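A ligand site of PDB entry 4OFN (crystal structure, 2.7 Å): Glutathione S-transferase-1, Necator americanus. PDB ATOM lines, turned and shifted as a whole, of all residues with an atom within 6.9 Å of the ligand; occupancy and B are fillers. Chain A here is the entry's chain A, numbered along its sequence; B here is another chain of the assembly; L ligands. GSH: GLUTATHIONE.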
ATOM      1  N   TYR A   8     -22.927 -25.589  17.094  1.00  0.00           N
ATOM      2  CA  TYR A   8     -21.556 -25.150  17.363  1.00  0.00           C
ATOM      3  C   TYR A   8     -21.278 -23.916  16.492  1.00  0.00           C
ATOM      4  O   TYR A   8     -22.166 -23.463  15.773  1.00  0.00           O
ATOM      5  CB  TYR A   8     -20.578 -26.305  17.062  1.00  0.00           C
ATOM      6  CG  TYR A   8     -19.145 -26.045  17.460  1.00  0.00           C
ATOM      7  CD1 TYR A   8     -18.799 -25.773  18.787  1.00  0.00           C
ATOM      8  CD2 TYR A   8     -18.116 -26.080  16.521  1.00  0.00           C
ATOM      9  CE1 TYR A   8     -17.492 -25.537  19.151  1.00  0.00           C
ATOM     10  CE2 TYR A   8     -16.796 -25.839  16.885  1.00  0.00           C
ATOM     11  CZ  TYR A   8     -16.502 -25.569  18.197  1.00  0.00           C
ATOM     12  OH  TYR A   8     -15.196 -25.333  18.562  1.00  0.00           O
ATOM     13  N   PHE A   9     -20.077 -23.333  16.600  1.00  0.00           N
ATOM     14  CA  PHE A   9     -19.690 -22.201  15.741  1.00  0.00           C
ATOM     15  C   PHE A   9     -19.385 -22.634  14.307  1.00  0.00           C
ATOM     16  O   PHE A   9     -19.269 -23.823  14.016  1.00  0.00           O
ATOM     17  CB  PHE A   9     -18.497 -21.466  16.334  1.00  0.00           C
ATOM     18  CG  PHE A   9     -18.779 -20.798  17.651  1.00  0.00           C
ATOM     19  CD1 PHE A   9     -19.749 -19.807  17.729  1.00  0.00           C
ATOM     20  CD2 PHE A   9     -18.085 -21.141  18.800  1.00  0.00           C
ATOM     21  CE1 PHE A   9     -20.024 -19.186  18.933  1.00  0.00           C
ATOM     22  CE2 PHE A   9     -18.359 -20.524  20.013  1.00  0.00           C
ATOM     23  CZ  PHE A   9     -19.326 -19.541  20.077  1.00  0.00           C
ATOM     24  N   ILE A  11     -17.104 -23.413  12.306  1.00  0.00           N
ATOM     25  CA  ILE A  11     -15.724 -23.893  12.304  1.00  0.00           C
ATOM     26  C   ILE A  11     -15.759 -25.382  12.636  1.00  0.00           C
ATOM     27  O   ILE A  11     -16.782 -25.912  13.068  1.00  0.00           O
ATOM     28  CB  ILE A  11     -14.841 -23.170  13.346  1.00  0.00           C
ATOM     29  CG1 ILE A  11     -15.587 -23.004  14.677  1.00  0.00           C
ATOM     30  CG2 ILE A  11     -14.359 -21.819  12.829  1.00  0.00           C
ATOM     31  CD1 ILE A  11     -14.698 -22.560  15.812  1.00  0.00           C
ATOM     32  N   ALA A  14     -14.011 -28.338  18.083  1.00  0.00           N
ATOM     33  CA  ALA A  14     -14.430 -29.466  18.916  1.00  0.00           C
ATOM     34  C   ALA A  14     -15.744 -30.126  18.468  1.00  0.00           C
ATOM     35  O   ALA A  14     -16.142 -31.151  19.021  1.00  0.00           O
ATOM     36  CB  ALA A  14     -14.549 -29.011  20.362  1.00  0.00           C
ATOM     37  N   PHE A  39     -25.105 -16.926  19.078  1.00  0.00           N
ATOM     38  CA  PHE A  39     -24.686 -17.691  20.258  1.00  0.00           C
ATOM     39  C   PHE A  39     -25.095 -16.978  21.550  1.00  0.00           C
ATOM     40  O   PHE A  39     -25.511 -17.626  22.515  1.00  0.00           O
ATOM     41  CB  PHE A  39     -23.176 -17.938  20.242  1.00  0.00           C
ATOM     42  CG  PHE A  39     -22.635 -18.508  21.524  1.00  0.00           C
ATOM     43  CD1 PHE A  39     -22.883 -19.832  21.869  1.00  0.00           C
ATOM     44  CD2 PHE A  39     -21.877 -17.733  22.388  1.00  0.00           C
ATOM     45  CE1 PHE A  39     -22.387 -20.361  23.044  1.00  0.00           C
ATOM     46  CE2 PHE A  39     -21.385 -18.251  23.570  1.00  0.00           C
ATOM     47  CZ  PHE A  39     -21.636 -19.567  23.896  1.00  0.00           C
ATOM     48  N   LYS A  43     -27.105 -18.835  24.370  1.00  0.00           N
ATOM     49  CA  LYS A  43     -26.144 -19.221  25.421  1.00  0.00           C
ATOM     50  C   LYS A  43     -26.760 -19.504  26.789  1.00  0.00           C
ATOM     51  O   LYS A  43     -26.418 -20.506  27.416  1.00  0.00           O
ATOM     52  CB  LYS A  43     -25.037 -18.164  25.564  1.00  0.00           C
ATOM     53  CG  LYS A  43     -24.252 -18.219  26.875  1.00  0.00           C
ATOM     54  CD  LYS A  43     -22.988 -17.370  26.784  1.00  0.00           C
ATOM     55  CE  LYS A  43     -22.071 -17.559  27.955  1.00  0.00           C
ATOM     56  NZ  LYS A  43     -22.668 -17.109  29.236  1.00  0.00           N
ATOM     57  N   PHE A  48     -24.113 -25.759  29.998  1.00  0.00           N
ATOM     58  CA  PHE A  48     -22.998 -25.076  30.658  1.00  0.00           C
ATOM     59  C   PHE A  48     -22.615 -23.772  29.958  1.00  0.00           C
ATOM     60  O   PHE A  48     -21.492 -23.290  30.100  1.00  0.00           O
ATOM     61  CB  PHE A  48     -21.790 -26.013  30.753  1.00  0.00           C
ATOM     62  CG  PHE A  48     -22.125 -27.380  31.316  1.00  0.00           C
ATOM     63  CD1 PHE A  48     -22.395 -27.537  32.661  1.00  0.00           C
ATOM     64  CD2 PHE A  48     -22.149 -28.489  30.494  1.00  0.00           C
ATOM     65  CE1 PHE A  48     -22.695 -28.788  33.182  1.00  0.00           C
ATOM     66  CE2 PHE A  48     -22.455 -29.744  31.004  1.00  0.00           C
ATOM     67  CZ  PHE A  48     -22.729 -29.889  32.355  1.00  0.00           C
ATOM     68  N   GLY A  49     -23.568 -23.194  29.229  1.00  0.00           N
ATOM     69  CA  GLY A  49     -23.379 -21.908  28.554  1.00  0.00           C
ATOM     70  C   GLY A  49     -22.362 -21.941  27.427  1.00  0.00           C
ATOM     71  O   GLY A  49     -21.733 -20.923  27.132  1.00  0.00           O
ATOM     72  N   GLN A  50     -22.248 -23.097  26.784  1.00  0.00           N
ATOM     73  CA  GLN A  50     -21.143 -23.399  25.897  1.00  0.00           C
ATOM     74  C   GLN A  50     -21.571 -24.323  24.762  1.00  0.00           C
ATOM     75  O   GLN A  50     -22.539 -25.072  24.916  1.00  0.00           O
ATOM     76  CB  GLN A  50     -20.075 -24.158  26.678  1.00  0.00           C
ATOM     77  CG  GLN A  50     -18.612 -23.818  26.350  1.00  0.00           C
ATOM     78  CD  GLN A  50     -18.074 -22.620  27.091  1.00  0.00           C
ATOM     79  OE1 GLN A  50     -16.922 -22.648  27.560  1.00  0.00           O
ATOM     80  NE2 GLN A  50     -18.875 -21.575  27.221  1.00  0.00           N
ATOM     81  N   VAL A  51     -20.821 -24.311  23.669  1.00  0.00           N
ATOM     82  CA  VAL A  51     -21.004 -25.251  22.563  1.00  0.00           C
ATOM     83  C   VAL A  51     -19.694 -26.020  22.305  1.00  0.00           C
ATOM     84  O   VAL A  51     -18.608 -25.530  22.647  1.00  0.00           O
ATOM     85  CB  VAL A  51     -21.462 -24.531  21.268  1.00  0.00           C
ATOM     86  CG1 VAL A  51     -22.943 -24.190  21.346  1.00  0.00           C
ATOM     87  CG2 VAL A  51     -20.642 -23.282  21.003  1.00  0.00           C
ATOM     88  N   PRO A  52     -19.766 -27.220  21.707  1.00  0.00           N
ATOM     89  CA  PRO A  52     -20.891 -27.916  21.065  1.00  0.00           C
ATOM     90  C   PRO A  52     -21.961 -28.463  22.011  1.00  0.00           C
ATOM     91  O   PRO A  52     -21.679 -28.783  23.174  1.00  0.00           O
ATOM     92  CB  PRO A  52     -20.208 -29.081  20.353  1.00  0.00           C
ATOM     93  CG  PRO A  52     -19.050 -29.396  21.235  1.00  0.00           C
ATOM     94  CD  PRO A  52     -18.559 -28.070  21.731  1.00  0.00           C
ATOM     95  N   VAL A  53     -23.183 -28.559  21.496  1.00  0.00           N
ATOM     96  CA  VAL A  53     -24.309 -29.150  22.218  1.00  0.00           C
ATOM     97  C   VAL A  53     -25.088 -30.043  21.281  1.00  0.00           C
ATOM     98  O   VAL A  53     -25.522 -29.603  20.221  1.00  0.00           O
ATOM     99  CB  VAL A  53     -25.251 -28.066  22.792  1.00  0.00           C
ATOM    100  CG1 VAL A  53     -26.465 -28.684  23.462  1.00  0.00           C
ATOM    101  CG2 VAL A  53     -24.485 -27.178  23.763  1.00  0.00           C
ATOM    102  N   ALA A  62     -24.285 -31.593  26.392  1.00  0.00           N
ATOM    103  CA  ALA A  62     -23.111 -30.749  26.157  1.00  0.00           C
ATOM    104  C   ALA A  62     -21.810 -31.543  26.213  1.00  0.00           C
ATOM    105  O   ALA A  62     -21.831 -32.749  26.473  1.00  0.00           O
ATOM    106  CB  ALA A  62     -23.083 -29.601  27.163  1.00  0.00           C
ATOM    107  N   GLN A  63     -20.693 -30.865  25.956  1.00  0.00           N
ATOM    108  CA  GLN A  63     -19.322 -31.424  26.053  1.00  0.00           C
ATOM    109  C   GLN A  63     -18.941 -32.397  24.924  1.00  0.00           C
ATOM    110  O   GLN A  63     -19.508 -33.481  24.810  1.00  0.00           O
ATOM    111  CB  GLN A  63     -19.059 -32.050  27.425  1.00  0.00           C
ATOM    112  CG  GLN A  63     -19.049 -31.039  28.571  1.00  0.00           C
ATOM    113  CD  GLN A  63     -17.775 -30.212  28.657  1.00  0.00           C
ATOM    114  OE1 GLN A  63     -16.882 -30.351  27.815  1.00  0.00           O
ATOM    115  NE2 GLN A  63     -17.691 -29.360  29.661  1.00  0.00           N
ATOM    116  N   SER A  64     -17.952 -32.002  24.123  1.00  0.00           N
ATOM    117  CA  SER A  64     -17.548 -32.716  22.909  1.00  0.00           C
ATOM    118  C   SER A  64     -17.169 -34.177  23.117  1.00  0.00           C
ATOM    119  O   SER A  64     -17.539 -35.037  22.314  1.00  0.00           O
ATOM    120  CB  SER A  64     -16.390 -31.998  22.218  1.00  0.00           C
ATOM    121  OG  SER A  64     -15.382 -31.628  23.141  1.00  0.00           O
ATOM    122  N   LEU A  65     -16.435 -34.468  24.194  1.00  0.00           N
ATOM    123  CA  LEU A  65     -16.031 -35.843  24.492  1.00  0.00           C
ATOM    124  C   LEU A  65     -17.231 -36.717  24.784  1.00  0.00           C
ATOM    125  O   LEU A  65     -17.324 -37.849  24.299  1.00  0.00           O
ATOM    126  CB  LEU A  65     -15.044 -35.882  25.676  1.00  0.00           C
ATOM    127  CG  LEU A  65     -13.727 -35.128  25.498  1.00  0.00           C
ATOM    128  CD1 LEU A  65     -12.799 -35.349  26.675  1.00  0.00           C
ATOM    129  CD2 LEU A  65     -13.037 -35.525  24.192  1.00  0.00           C
ATOM    130  N   ILE A  67     -20.325 -36.025  23.829  1.00  0.00           N
ATOM    131  CA  ILE A  67     -21.088 -36.076  22.576  1.00  0.00           C
ATOM    132  C   ILE A  67     -20.523 -37.144  21.651  1.00  0.00           C
ATOM    133  O   ILE A  67     -21.246 -38.024  21.189  1.00  0.00           O
ATOM    134  CB  ILE A  67     -21.109 -34.703  21.854  1.00  0.00           C
ATOM    135  CG1 ILE A  67     -21.925 -33.691  22.663  1.00  0.00           C
ATOM    136  CG2 ILE A  67     -21.697 -34.835  20.455  1.00  0.00           C
ATOM    137  CD1 ILE A  67     -21.585 -32.242  22.361  1.00  0.00           C
ATOM    138  N   LYS A 103      -2.584 -24.703  23.847  1.00  0.00           N
ATOM    139  CA  LYS A 103      -3.566 -23.616  23.783  1.00  0.00           C
ATOM    140  C   LYS A 103      -2.878 -22.290  23.476  1.00  0.00           C
ATOM    141  O   LYS A 103      -3.276 -21.576  22.569  1.00  0.00           O
ATOM    142  CB  LYS A 103      -4.348 -23.500  25.108  1.00  0.00           C
ATOM    143  CG  LYS A 103      -5.749 -22.921  24.970  1.00  0.00           C
ATOM    144  CD  LYS A 103      -6.790 -24.025  25.151  1.00  0.00           C
ATOM    145  CE  LYS A 103      -7.043 -24.384  26.623  1.00  0.00           C
ATOM    146  NZ  LYS A 103      -8.494 -24.539  26.956  1.00  0.00           N
ATOM    147  N   TYR A 107      -4.357 -20.732  19.822  1.00  0.00           N
ATOM    148  CA  TYR A 107      -5.145 -19.488  19.786  1.00  0.00           C
ATOM    149  C   TYR A 107      -4.384 -18.302  19.189  1.00  0.00           C
ATOM    150  O   TYR A 107      -4.999 -17.369  18.678  1.00  0.00           O
ATOM    151  CB  TYR A 107      -5.656 -19.111  21.197  1.00  0.00           C
ATOM    152  CG  TYR A 107      -6.871 -19.886  21.705  1.00  0.00           C
ATOM    153  CD1 TYR A 107      -7.503 -20.874  20.932  1.00  0.00           C
ATOM    154  CD2 TYR A 107      -7.415 -19.614  22.961  1.00  0.00           C
ATOM    155  CE1 TYR A 107      -8.605 -21.567  21.403  1.00  0.00           C
ATOM    156  CE2 TYR A 107      -8.520 -20.299  23.447  1.00  0.00           C
ATOM    157  CZ  TYR A 107      -9.118 -21.278  22.662  1.00  0.00           C
ATOM    158  OH  TYR A 107     -10.211 -21.954  23.138  1.00  0.00           O
ATOM    159  N   MET A 112      -7.214 -15.550  18.160  1.00  0.00           N
ATOM    160  CA  MET A 112      -8.187 -15.344  19.237  1.00  0.00           C
ATOM    161  C   MET A 112      -7.505 -14.748  20.477  1.00  0.00           C
ATOM    162  O   MET A 112      -8.178 -14.264  21.385  1.00  0.00           O
ATOM    163  CB  MET A 112      -8.869 -16.663  19.613  1.00  0.00           C
ATOM    164  CG  MET A 112     -10.372 -16.516  19.828  1.00  0.00           C
ATOM    165  SD  MET A 112     -11.131 -17.918  20.681  1.00  0.00           S
ATOM    166  CE  MET A 112     -12.595 -17.160  21.406  1.00  0.00           C
ATOM    167  N   ASP B  93     -16.597 -33.771  32.774  1.00  0.00           N
ATOM    168  CA  ASP B  93     -15.715 -32.950  31.932  1.00  0.00           C
ATOM    169  C   ASP B  93     -15.816 -31.471  32.299  1.00  0.00           C
ATOM    170  O   ASP B  93     -14.808 -30.767  32.273  1.00  0.00           O
ATOM    171  CB  ASP B  93     -16.040 -33.138  30.440  1.00  0.00           C
ATOM    172  CG  ASP B  93     -15.564 -34.475  29.895  1.00  0.00           C
ATOM    173  OD1 ASP B  93     -14.561 -35.032  30.425  1.00  0.00           O
ATOM    174  OD2 ASP B  93     -16.176 -34.957  28.930  1.00  0.00           O
ATOM    175  N   GLN B  94     -17.024 -31.023  32.647  1.00  0.00           N
ATOM    176  CA  GLN B  94     -17.227 -29.655  33.114  1.00  0.00           C
ATOM    177  C   GLN B  94     -16.482 -29.438  34.435  1.00  0.00           C
ATOM    178  O   GLN B  94     -15.949 -28.357  34.677  1.00  0.00           O
ATOM    179  CB  GLN B  94     -18.717 -29.348  33.299  1.00  0.00           C
ATOM    180  CG  GLN B  94     -19.035 -27.892  33.604  1.00  0.00           C
ATOM    181  CD  GLN B  94     -18.760 -26.969  32.434  1.00  0.00           C
ATOM    182  OE1 GLN B  94     -18.954 -27.329  31.275  1.00  0.00           O
ATOM    183  NE2 GLN B  94     -18.310 -25.753  32.730  1.00  0.00           N
ATOM    184  N   ASP B  97     -12.782 -29.075  33.411  1.00  0.00           N
ATOM    185  CA  ASP B  97     -12.538 -27.703  32.910  1.00  0.00           C
ATOM    186  C   ASP B  97     -12.476 -26.711  34.061  1.00  0.00           C
ATOM    187  O   ASP B  97     -11.736 -25.725  34.011  1.00  0.00           O
ATOM    188  CB  ASP B  97     -13.618 -27.270  31.914  1.00  0.00           C
ATOM    189  CG  ASP B  97     -13.618 -28.095  30.640  1.00  0.00           C
ATOM    190  OD1 ASP B  97     -12.584 -28.734  30.323  1.00  0.00           O
ATOM    191  OD2 ASP B  97     -14.654 -28.109  29.941  1.00  0.00           O
ATOM    192  N   LYS B 131     -19.698 -19.726  38.789  1.00  0.00           N
ATOM    193  CA  LYS B 131     -20.126 -20.238  37.488  1.00  0.00           C
ATOM    194  C   LYS B 131     -20.398 -21.744  37.541  1.00  0.00           C
ATOM    195  O   LYS B 131     -21.406 -22.208  37.009  1.00  0.00           O
ATOM    196  CB  LYS B 131     -19.066 -19.907  36.423  1.00  0.00           C
ATOM    197  CG  LYS B 131     -19.009 -20.853  35.228  1.00  0.00           C
ATOM    198  CD  LYS B 131     -17.974 -20.405  34.209  1.00  0.00           C
ATOM    199  CE  LYS B 131     -17.680 -21.493  33.198  1.00  0.00           C
ATOM    200  NZ  LYS B 131     -16.662 -21.057  32.210  1.00  0.00           N
HETATM  201  N1  GSH L   1     -14.550 -28.676  27.007  1.00  0.00           N
HETATM  202  CA1 GSH L   1     -15.617 -28.005  26.297  1.00  0.00           C
HETATM  203  C1  GSH L   1     -16.082 -28.818  25.119  1.00  0.00           C
HETATM  204  O11 GSH L   1     -17.305 -28.898  24.924  1.00  0.00           O
HETATM  205  O12 GSH L   1     -15.230 -29.360  24.388  1.00  0.00           O
HETATM  206  CB1 GSH L   1     -15.114 -26.670  25.791  1.00  0.00           C
HETATM  207  CG1 GSH L   1     -16.199 -25.973  24.972  1.00  0.00           C
HETATM  208  CD1 GSH L   1     -15.833 -24.528  24.775  1.00  0.00           C
HETATM  209  OE1 GSH L   1     -14.996 -23.994  25.481  1.00  0.00           O
HETATM  210  N2  GSH L   1     -16.464 -23.899  23.769  1.00  0.00           N
HETATM  211  CA2 GSH L   1     -16.099 -22.550  23.372  1.00  0.00           C
HETATM  212  C2  GSH L   1     -17.154 -21.519  23.673  1.00  0.00           C
HETATM  213  O2  GSH L   1     -18.299 -21.851  23.917  1.00  0.00           O
HETATM  214  CB2 GSH L   1     -15.739 -22.551  21.893  1.00  0.00           C
HETATM  215  SG2 GSH L   1     -14.541 -21.256  21.540  1.00  0.00           S
HETATM  216  N3  GSH L   1     -16.733 -20.251  23.675  1.00  0.00           N
HETATM  217  CA3 GSH L   1     -17.594 -19.128  23.985  1.00  0.00           C
HETATM  218  C3  GSH L   1     -17.325 -18.606  25.374  1.00  0.00           C
HETATM  219  O31 GSH L   1     -17.853 -19.188  26.366  1.00  0.00           O
HETATM  220  O32 GSH L   1     -16.570 -17.613  25.480  1.00  0.00           O
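An oxygen (O31) of the ligand is in hydrogen-bond range of the side-chain amide nitrogen (NE2) of Gln 50, 2.7 Å away.
A nitrogen (N2) of the ligand is in hydrogen-bond range of the backbone carbonyl oxygen (O) of Val 51 (2.9 Å).
The backbone NH (N) of Ser 64 sits at hydrogen-bond distance from an oxygen (O11) of the ligand, at 3.3 Å.
A nitrogen (N1) of the ligand sits at hydrogen-bond distance from the side-chain amide oxygen (OE1) of Gln 63, at 3.0 Å.
The side-chain hydroxyl (OG) of Ser 64 sits at hydrogen-bond distance from an oxygen (O12) of the ligand (2.6 Å).
The side-chain carboxylate (OD2) of Asp 97 of chain B is in salt-bridge range of a nitrogen (N1) of the ligand, at 3.0 Å.
The side-chain amide oxygen (OE1) of Gln 94 of chain B sits at hydrogen-bond distance from the side-chain amide nitrogen (NE2) of Gln 63.
The side-chain amide nitrogen of Gln 63 is in hydrogen-bond range of the side-chain carboxylate of Asp 97 of chain B (3.3 Å).
Phe 9 touches the ligand.
Phe 39 touches the ligand (CE2 to CA3, 3.9 Å).
Pro 52 touches the ligand (CD to O11, 3.5 Å).
Eight residues have an atom within 4 Å of the ligand: Phe 9, Phe 39, Gln 50, Val 51, Pro 52, Gln 63, Ser 64 and Asp 97 of chain B.
Along chain A the residues within 4 Å of the ligand span positions 9 to 64.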
